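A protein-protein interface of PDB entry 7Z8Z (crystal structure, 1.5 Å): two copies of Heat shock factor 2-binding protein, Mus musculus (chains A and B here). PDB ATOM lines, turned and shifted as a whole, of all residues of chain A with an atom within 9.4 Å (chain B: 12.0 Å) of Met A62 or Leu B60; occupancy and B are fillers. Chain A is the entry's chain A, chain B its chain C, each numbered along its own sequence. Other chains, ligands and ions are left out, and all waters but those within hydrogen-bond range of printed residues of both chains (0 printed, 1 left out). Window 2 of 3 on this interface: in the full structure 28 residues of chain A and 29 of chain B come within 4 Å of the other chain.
Printed residues of chain B that touch a printed residue of chain A: Lys B53, Glu B54, Glu B56, Leu B57, Leu B60 and Ile B61. Hydrophobic or aromatic side chains of chain B that line the printed part of chain A: Leu B57, Leu B60 and Ile B61. Hydrophobic or aromatic side chains of chain A that line the printed part of chain B: Leu A57, Leu A60 and Met A62.
Of chain B, only Leu B60 comes within 4 Å of Met A62. Of chain A, only Leu A60 and Met A62 come within 4 Å of Leu B60. Of chain B, only Lys B53 (3.7 Å), Glu B56 (3.96 Å) and Leu B57 (3.7 Å) come within 4 Å of Leu A57. Leu A60 touches just these residues of chain B: Leu B60 (3.6 Å) and Ile B61 (3.9 Å). No residue of chain B comes within 4 Å of Ile A61. No residue of chain B comes within 4 Å of Asp A63. Of the printed residues of chain A, Ile B61 touches Leu A60. Of the printed residues of chain A, Glu B54 touches Lys A53 (3.8 Å). Of the printed residues of chain B, Lys A53 touches Lys B53, Glu B54 and Leu B57. The nearest residue of chain B that does not touch Met A62 is Glu B56 (6.6 Å).
Lys B53 touches its own counterpart, Lys A53. Leu B57 touches its own counterpart, Leu A57. Leu B60 touches its own counterpart, Leu A60. Leu A60 touches Ile B61, but with the chains exchanged Ile A61 does not touch Leu B60 (6.7 Å). Positions printed for both chains: 53, 56, 57, 58, 59, 60 and 61.
Among the printed residues, pairs that only touch across the chains: Lys A53 with Lys B53 (3.8 Å), Lys A53 with Glu B54 (3.8 Å), Lys A53 with Leu B57 (3.7 Å), Glu A56 with Leu B57 (3.3 Å), Leu A57 with Lys B53 (3.7 Å), Leu A57 with Glu B56 (3.96 Å), Leu A57 with Leu B57 (3.7 Å), Leu A60 with Leu B60 (3.6 Å), Leu A60 with Ile B61 (3.9 Å) and Met A62 with Leu B60 (3.9 Å).
OE1 of Glu A56 is in salt-bridge range of NZ of Lys A53 (3.5 Å). NZ of Lys B53 lies within salt-bridge range of OE1 of Glu B56.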
ATOM      1  N   LYS A  53      30.498  -8.065   3.033  1.00  0.00           N
ATOM      2  CA  LYS A  53      29.328  -8.817   2.589  1.00  0.00           C
ATOM      3  C   LYS A  53      28.057  -7.986   2.737  1.00  0.00           C
ATOM      4  O   LYS A  53      27.092  -8.190   1.993  1.00  0.00           O
ATOM      5  CB  LYS A  53      29.206 -10.116   3.378  1.00  0.00           C
ATOM      6  CG  LYS A  53      28.639 -11.276   2.572  1.00  0.00           C
ATOM      7  CD  LYS A  53      29.625 -11.726   1.500  1.00  0.00           C
ATOM      8  CE  LYS A  53      29.012 -12.792   0.598  1.00  0.00           C
ATOM      9  NZ  LYS A  53      29.934 -13.183  -0.510  1.00  0.00           N
ATOM     10  N   GLU A  56      27.990  -5.526  -0.250  1.00  0.00           N
ATOM     11  CA  GLU A  56      27.520  -6.165  -1.476  1.00  0.00           C
ATOM     12  C   GLU A  56      25.998  -6.231  -1.510  1.00  0.00           C
ATOM     13  O   GLU A  56      25.385  -6.031  -2.564  1.00  0.00           O
ATOM     14  CB  GLU A  56      28.118  -7.565  -1.602  1.00  0.00           C
ATOM     15  CG  GLU A  56      29.577  -7.582  -2.024  1.00  0.00           C
ATOM     16  CD  GLU A  56      30.149  -8.985  -2.089  1.00  0.00           C
ATOM     17  OE1 GLU A  56      29.891  -9.777  -1.157  1.00  0.00           O
ATOM     18  OE2 GLU A  56      30.851  -9.299  -3.074  1.00  0.00           O
ATOM     19  N   LEU A  57      25.370  -6.507  -0.364  1.00  0.00           N
ATOM     20  CA  LEU A  57      23.914  -6.533  -0.307  1.00  0.00           C
ATOM     21  C   LEU A  57      23.325  -5.133  -0.423  1.00  0.00           C
ATOM     22  O   LEU A  57      22.213  -4.970  -0.941  1.00  0.00           O
ATOM     23  CB  LEU A  57      23.461  -7.196   0.991  1.00  0.00           C
ATOM     24  CG  LEU A  57      23.761  -8.687   1.121  1.00  0.00           C
ATOM     25  CD1 LEU A  57      23.660  -9.134   2.568  1.00  0.00           C
ATOM     26  CD2 LEU A  57      22.811  -9.489   0.239  1.00  0.00           C
ATOM     27  N   GLU A  58      24.055  -4.113   0.045  1.00  0.00           N
ATOM     28  CA  GLU A  58      23.543  -2.746  -0.018  1.00  0.00           C
ATOM     29  C   GLU A  58      23.622  -2.188  -1.434  1.00  0.00           C
ATOM     30  O   GLU A  58      22.776  -1.377  -1.829  1.00  0.00           O
ATOM     31  CB  GLU A  58      24.321  -1.854   0.950  1.00  0.00           C
ATOM     32  CG  GLU A  58      23.772  -0.442   1.107  1.00  0.00           C
ATOM     33  CD  GLU A  58      24.294   0.523   0.054  1.00  0.00           C
ATOM     34  OE1 GLU A  58      25.262   0.177  -0.656  1.00  0.00           O
ATOM     35  OE2 GLU A  58      23.735   1.634  -0.063  1.00  0.00           O
ATOM     36  N   GLN A  59      24.633  -2.593  -2.206  1.00  0.00           N
ATOM     37  CA  GLN A  59      24.770  -2.136  -3.584  1.00  0.00           C
ATOM     38  C   GLN A  59      23.904  -2.922  -4.560  1.00  0.00           C
ATOM     39  O   GLN A  59      23.810  -2.538  -5.732  1.00  0.00           O
ATOM     40  CB  GLN A  59      26.234  -2.228  -4.028  1.00  0.00           C
ATOM     41  CG  GLN A  59      27.180  -1.307  -3.279  1.00  0.00           C
ATOM     42  CD  GLN A  59      28.629  -1.495  -3.698  1.00  0.00           C
ATOM     43  OE1 GLN A  59      28.931  -2.277  -4.600  1.00  0.00           O
ATOM     44  NE2 GLN A  59      29.531  -0.779  -3.038  1.00  0.00           N
ATOM     45  N   LEU A  60      23.275  -4.005  -4.113  1.00  0.00           N
ATOM     46  CA  LEU A  60      22.487  -4.846  -5.002  1.00  0.00           C
ATOM     47  C   LEU A  60      21.079  -4.288  -5.156  1.00  0.00           C
ATOM     48  O   LEU A  60      20.423  -3.947  -4.166  1.00  0.00           O
ATOM     49  CB  LEU A  60      22.431  -6.276  -4.465  1.00  0.00           C
ATOM     50  CG  LEU A  60      21.627  -7.276  -5.292  1.00  0.00           C
ATOM     51  CD1 LEU A  60      22.234  -7.451  -6.673  1.00  0.00           C
ATOM     52  CD2 LEU A  60      21.541  -8.617  -4.565  1.00  0.00           C
ATOM     53  N   ILE A  61      20.620  -4.191  -6.400  1.00  0.00           N
ATOM     54  CA  ILE A  61      19.254  -3.795  -6.717  1.00  0.00           C
ATOM     55  C   ILE A  61      18.466  -5.077  -6.950  1.00  0.00           C
ATOM     56  O   ILE A  61      18.646  -5.754  -7.968  1.00  0.00           O
ATOM     57  CB  ILE A  61      19.198  -2.865  -7.936  1.00  0.00           C
ATOM     58  CG1 ILE A  61      20.082  -1.639  -7.693  1.00  0.00           C
ATOM     59  CG2 ILE A  61      17.768  -2.442  -8.210  1.00  0.00           C
ATOM     60  CD1 ILE A  61      20.096  -0.644  -8.831  1.00  0.00           C
ATOM     61  N   MET A  62      17.591  -5.417  -5.999  1.00  0.00           N
ATOM     62  CA  MET A  62      16.889  -6.694  -6.041  1.00  0.00           C
ATOM     63  C   MET A  62      15.418  -6.580  -5.663  1.00  0.00           C
ATOM     64  O   MET A  62      14.751  -7.614  -5.530  1.00  0.00           O
ATOM     65  CB  MET A  62      17.581  -7.711  -5.115  1.00  0.00           C
ATOM     66  CG  MET A  62      18.058  -7.138  -3.781  1.00  0.00           C
ATOM     67  SD  MET A  62      16.740  -6.568  -2.686  1.00  0.00           S
ATOM     68  CE  MET A  62      15.853  -8.094  -2.385  1.00  0.00           C
ATOM     69  N   ASP A  63      14.893  -5.373  -5.483  1.00  0.00           N
ATOM     70  CA  ASP A  63      13.476  -5.196  -5.187  1.00  0.00           C
ATOM     71  C   ASP A  63      13.009  -3.787  -5.546  1.00  0.00           C
ATOM     72  O   ASP A  63      13.757  -2.995  -6.120  1.00  0.00           O
ATOM     73  CB  ASP A  63      13.195  -5.483  -3.710  1.00  0.00           C
ATOM     74  CG  ASP A  63      13.934  -4.542  -2.776  1.00  0.00           C
ATOM     75  OD1 ASP A  63      14.704  -3.689  -3.263  1.00  0.00           O
ATOM     76  OD2 ASP A  63      13.741  -4.661  -1.547  1.00  0.00           O
ATOM     77  OXT ASP A  63      11.868  -3.411  -5.278  1.00  0.00           O
ATOM     78  N   GLU B  51      27.989 -15.782   7.857  1.00  0.00           N
ATOM     79  CA  GLU B  51      27.449 -16.926   7.129  1.00  0.00           C
ATOM     80  C   GLU B  51      26.008 -16.677   6.699  1.00  0.00           C
ATOM     81  O   GLU B  51      25.590 -17.117   5.622  1.00  0.00           O
ATOM     82  CB  GLU B  51      27.545 -18.190   7.985  1.00  0.00           C
ATOM     83  CG  GLU B  51      28.957 -18.729   8.131  1.00  0.00           C
ATOM     84  CD  GLU B  51      29.041 -19.902   9.088  1.00  0.00           C
ATOM     85  OE1 GLU B  51      27.988 -20.313   9.621  1.00  0.00           O
ATOM     86  OE2 GLU B  51      30.162 -20.409   9.312  1.00  0.00           O
ATOM     87  N   ARG B  52      25.231 -15.974   7.526  1.00  0.00           N
ATOM     88  CA  ARG B  52      23.857 -15.661   7.148  1.00  0.00           C
ATOM     89  C   ARG B  52      23.820 -14.739   5.934  1.00  0.00           C
ATOM     90  O   ARG B  52      23.066 -14.976   4.982  1.00  0.00           O
ATOM     91  CB  ARG B  52      23.116 -15.026   8.323  1.00  0.00           C
ATOM     92  CG  ARG B  52      22.239 -15.993   9.104  1.00  0.00           C
ATOM     93  CD  ARG B  52      21.306 -15.255  10.059  1.00  0.00           C
ATOM     94  NE  ARG B  52      22.037 -14.505  11.074  1.00  0.00           N
ATOM     95  CZ  ARG B  52      22.266 -14.943  12.303  1.00  0.00           C
ATOM     96  NH1 ARG B  52      21.816 -16.118  12.713  1.00  0.00           N
ATOM     97  NH2 ARG B  52      22.962 -14.183  13.145  1.00  0.00           N
ATOM     98  N   LYS B  53      24.627 -13.674   5.951  1.00  0.00           N
ATOM     99  CA  LYS B  53      24.656 -12.746   4.826  1.00  0.00           C
ATOM    100  C   LYS B  53      25.362 -13.340   3.612  1.00  0.00           C
ATOM    101  O   LYS B  53      25.150 -12.863   2.493  1.00  0.00           O
ATOM    102  CB  LYS B  53      25.330 -11.438   5.241  1.00  0.00           C
ATOM    103  CG  LYS B  53      24.623 -10.702   6.375  1.00  0.00           C
ATOM    104  CD  LYS B  53      23.198 -10.326   5.992  1.00  0.00           C
ATOM    105  CE  LYS B  53      22.468  -9.646   7.147  1.00  0.00           C
ATOM    106  NZ  LYS B  53      21.043  -9.361   6.805  1.00  0.00           N
ATOM    107  N   GLU B  54      26.202 -14.361   3.806  1.00  0.00           N
ATOM    108  CA  GLU B  54      26.783 -15.057   2.661  1.00  0.00           C
ATOM    109  C   GLU B  54      25.719 -15.844   1.905  1.00  0.00           C
ATOM    110  O   GLU B  54      25.672 -15.811   0.670  1.00  0.00           O
ATOM    111  CB  GLU B  54      27.907 -15.984   3.121  1.00  0.00           C
ATOM    112  CG  GLU B  54      29.207 -15.267   3.438  1.00  0.00           C
ATOM    113  CD  GLU B  54      30.240 -16.183   4.073  1.00  0.00           C
ATOM    114  OE1 GLU B  54      29.899 -17.345   4.380  1.00  0.00           O
ATOM    115  OE2 GLU B  54      31.390 -15.738   4.273  1.00  0.00           O
ATOM    116  N   GLN B  55      24.853 -16.556   2.632  1.00  0.00           N
ATOM    117  CA  GLN B  55      23.775 -17.294   1.983  1.00  0.00           C
ATOM    118  C   GLN B  55      22.721 -16.353   1.414  1.00  0.00           C
ATOM    119  O   GLN B  55      22.127 -16.647   0.371  1.00  0.00           O
ATOM    120  CB  GLN B  55      23.132 -18.267   2.973  1.00  0.00           C
ATOM    121  CG  GLN B  55      24.110 -19.194   3.681  1.00  0.00           C
ATOM    122  CD  GLN B  55      24.700 -20.249   2.763  1.00  0.00           C
ATOM    123  OE1 GLN B  55      24.673 -20.114   1.539  1.00  0.00           O
ATOM    124  NE2 GLN B  55      25.232 -21.313   3.353  1.00  0.00           N
ATOM    125  N   GLU B  56      22.474 -15.224   2.082  1.00  0.00           N
ATOM    126  CA  GLU B  56      21.499 -14.262   1.575  1.00  0.00           C
ATOM    127  C   GLU B  56      21.920 -13.735   0.208  1.00  0.00           C
ATOM    128  O   GLU B  56      21.110 -13.671  -0.724  1.00  0.00           O
ATOM    129  CB  GLU B  56      21.331 -13.111   2.568  1.00  0.00           C
ATOM    130  CG  GLU B  56      20.353 -12.036   2.116  1.00  0.00           C
ATOM    131  CD  GLU B  56      20.164 -10.938   3.151  1.00  0.00           C
ATOM    132  OE1 GLU B  56      20.672 -11.088   4.284  1.00  0.00           O
ATOM    133  OE2 GLU B  56      19.508  -9.924   2.830  1.00  0.00           O
ATOM    134  N   LEU B  57      23.192 -13.353   0.069  1.00  0.00           N
ATOM    135  CA  LEU B  57      23.668 -12.850  -1.216  1.00  0.00           C
ATOM    136  C   LEU B  57      23.648 -13.938  -2.281  1.00  0.00           C
ATOM    137  O   LEU B  57      23.433 -13.640  -3.462  1.00  0.00           O
ATOM    138  CB  LEU B  57      25.077 -12.280  -1.069  1.00  0.00           C
ATOM    139  CG  LEU B  57      25.649 -11.584  -2.305  1.00  0.00           C
ATOM    140  CD1 LEU B  57      24.811 -10.372  -2.687  1.00  0.00           C
ATOM    141  CD2 LEU B  57      27.102 -11.182  -2.068  1.00  0.00           C
ATOM    142  N   GLU B  58      23.862 -15.196  -1.890  1.00  0.00           N
ATOM    143  CA  GLU B  58      23.853 -16.283  -2.864  1.00  0.00           C
ATOM    144  C   GLU B  58      22.463 -16.481  -3.458  1.00  0.00           C
ATOM    145  O   GLU B  58      22.324 -16.709  -4.666  1.00  0.00           O
ATOM    146  CB  GLU B  58      24.347 -17.573  -2.211  1.00  0.00           C
ATOM    147  CG  GLU B  58      24.414 -18.765  -3.150  1.00  0.00           C
ATOM    148  CD  GLU B  58      24.949 -20.013  -2.470  1.00  0.00           C
ATOM    149  OE1 GLU B  58      25.317 -19.932  -1.278  1.00  0.00           O
ATOM    150  OE2 GLU B  58      25.001 -21.075  -3.128  1.00  0.00           O
ATOM    151  N   GLN B  59      21.423 -16.400  -2.626  1.00  0.00           N
ATOM    152  CA  GLN B  59      20.058 -16.567  -3.107  1.00  0.00           C
ATOM    153  C   GLN B  59      19.554 -15.355  -3.877  1.00  0.00           C
ATOM    154  O   GLN B  59      18.458 -15.419  -4.448  1.00  0.00           O
ATOM    155  CB  GLN B  59      19.118 -16.850  -1.932  1.00  0.00           C
ATOM    156  CG  GLN B  59      19.523 -18.040  -1.083  1.00  0.00           C
ATOM    157  CD  GLN B  59      19.566 -19.331  -1.876  1.00  0.00           C
ATOM    158  OE1 GLN B  59      18.656 -19.633  -2.650  1.00  0.00           O
ATOM    159  NE2 GLN B  59      20.634 -20.098  -1.693  1.00  0.00           N
ATOM    160  N   LEU B  60      20.318 -14.263  -3.909  1.00  0.00           N
ATOM    161  CA  LEU B  60      19.892 -13.039  -4.574  1.00  0.00           C
ATOM    162  C   LEU B  60      20.599 -12.795  -5.902  1.00  0.00           C
ATOM    163  O   LEU B  60      20.003 -12.196  -6.806  1.00  0.00           O
ATOM    164  CB  LEU B  60      20.125 -11.834  -3.658  1.00  0.00           C
ATOM    165  CG  LEU B  60      18.936 -11.376  -2.818  1.00  0.00           C
ATOM    166  CD1 LEU B  60      18.332 -12.521  -2.032  1.00  0.00           C
ATOM    167  CD2 LEU B  60      19.366 -10.245  -1.877  1.00  0.00           C
ATOM    168  N   ILE B  61      21.850 -13.230  -6.044  1.00  0.00           N
ATOM    169  CA  ILE B  61      22.570 -13.053  -7.301  1.00  0.00           C
ATOM    170  C   ILE B  61      22.647 -14.391  -8.035  1.00  0.00           C
ATOM    171  O   ILE B  61      22.576 -14.450  -9.264  1.00  0.00           O
ATOM    172  CB  ILE B  61      23.977 -12.470  -7.076  1.00  0.00           C
ATOM    173  CG1 ILE B  61      24.880 -13.485  -6.378  1.00  0.00           C
ATOM    174  CG2 ILE B  61      23.891 -11.188  -6.262  1.00  0.00           C
ATOM    175  CD1 ILE B  61      26.271 -12.952  -6.057  1.00  0.00           C
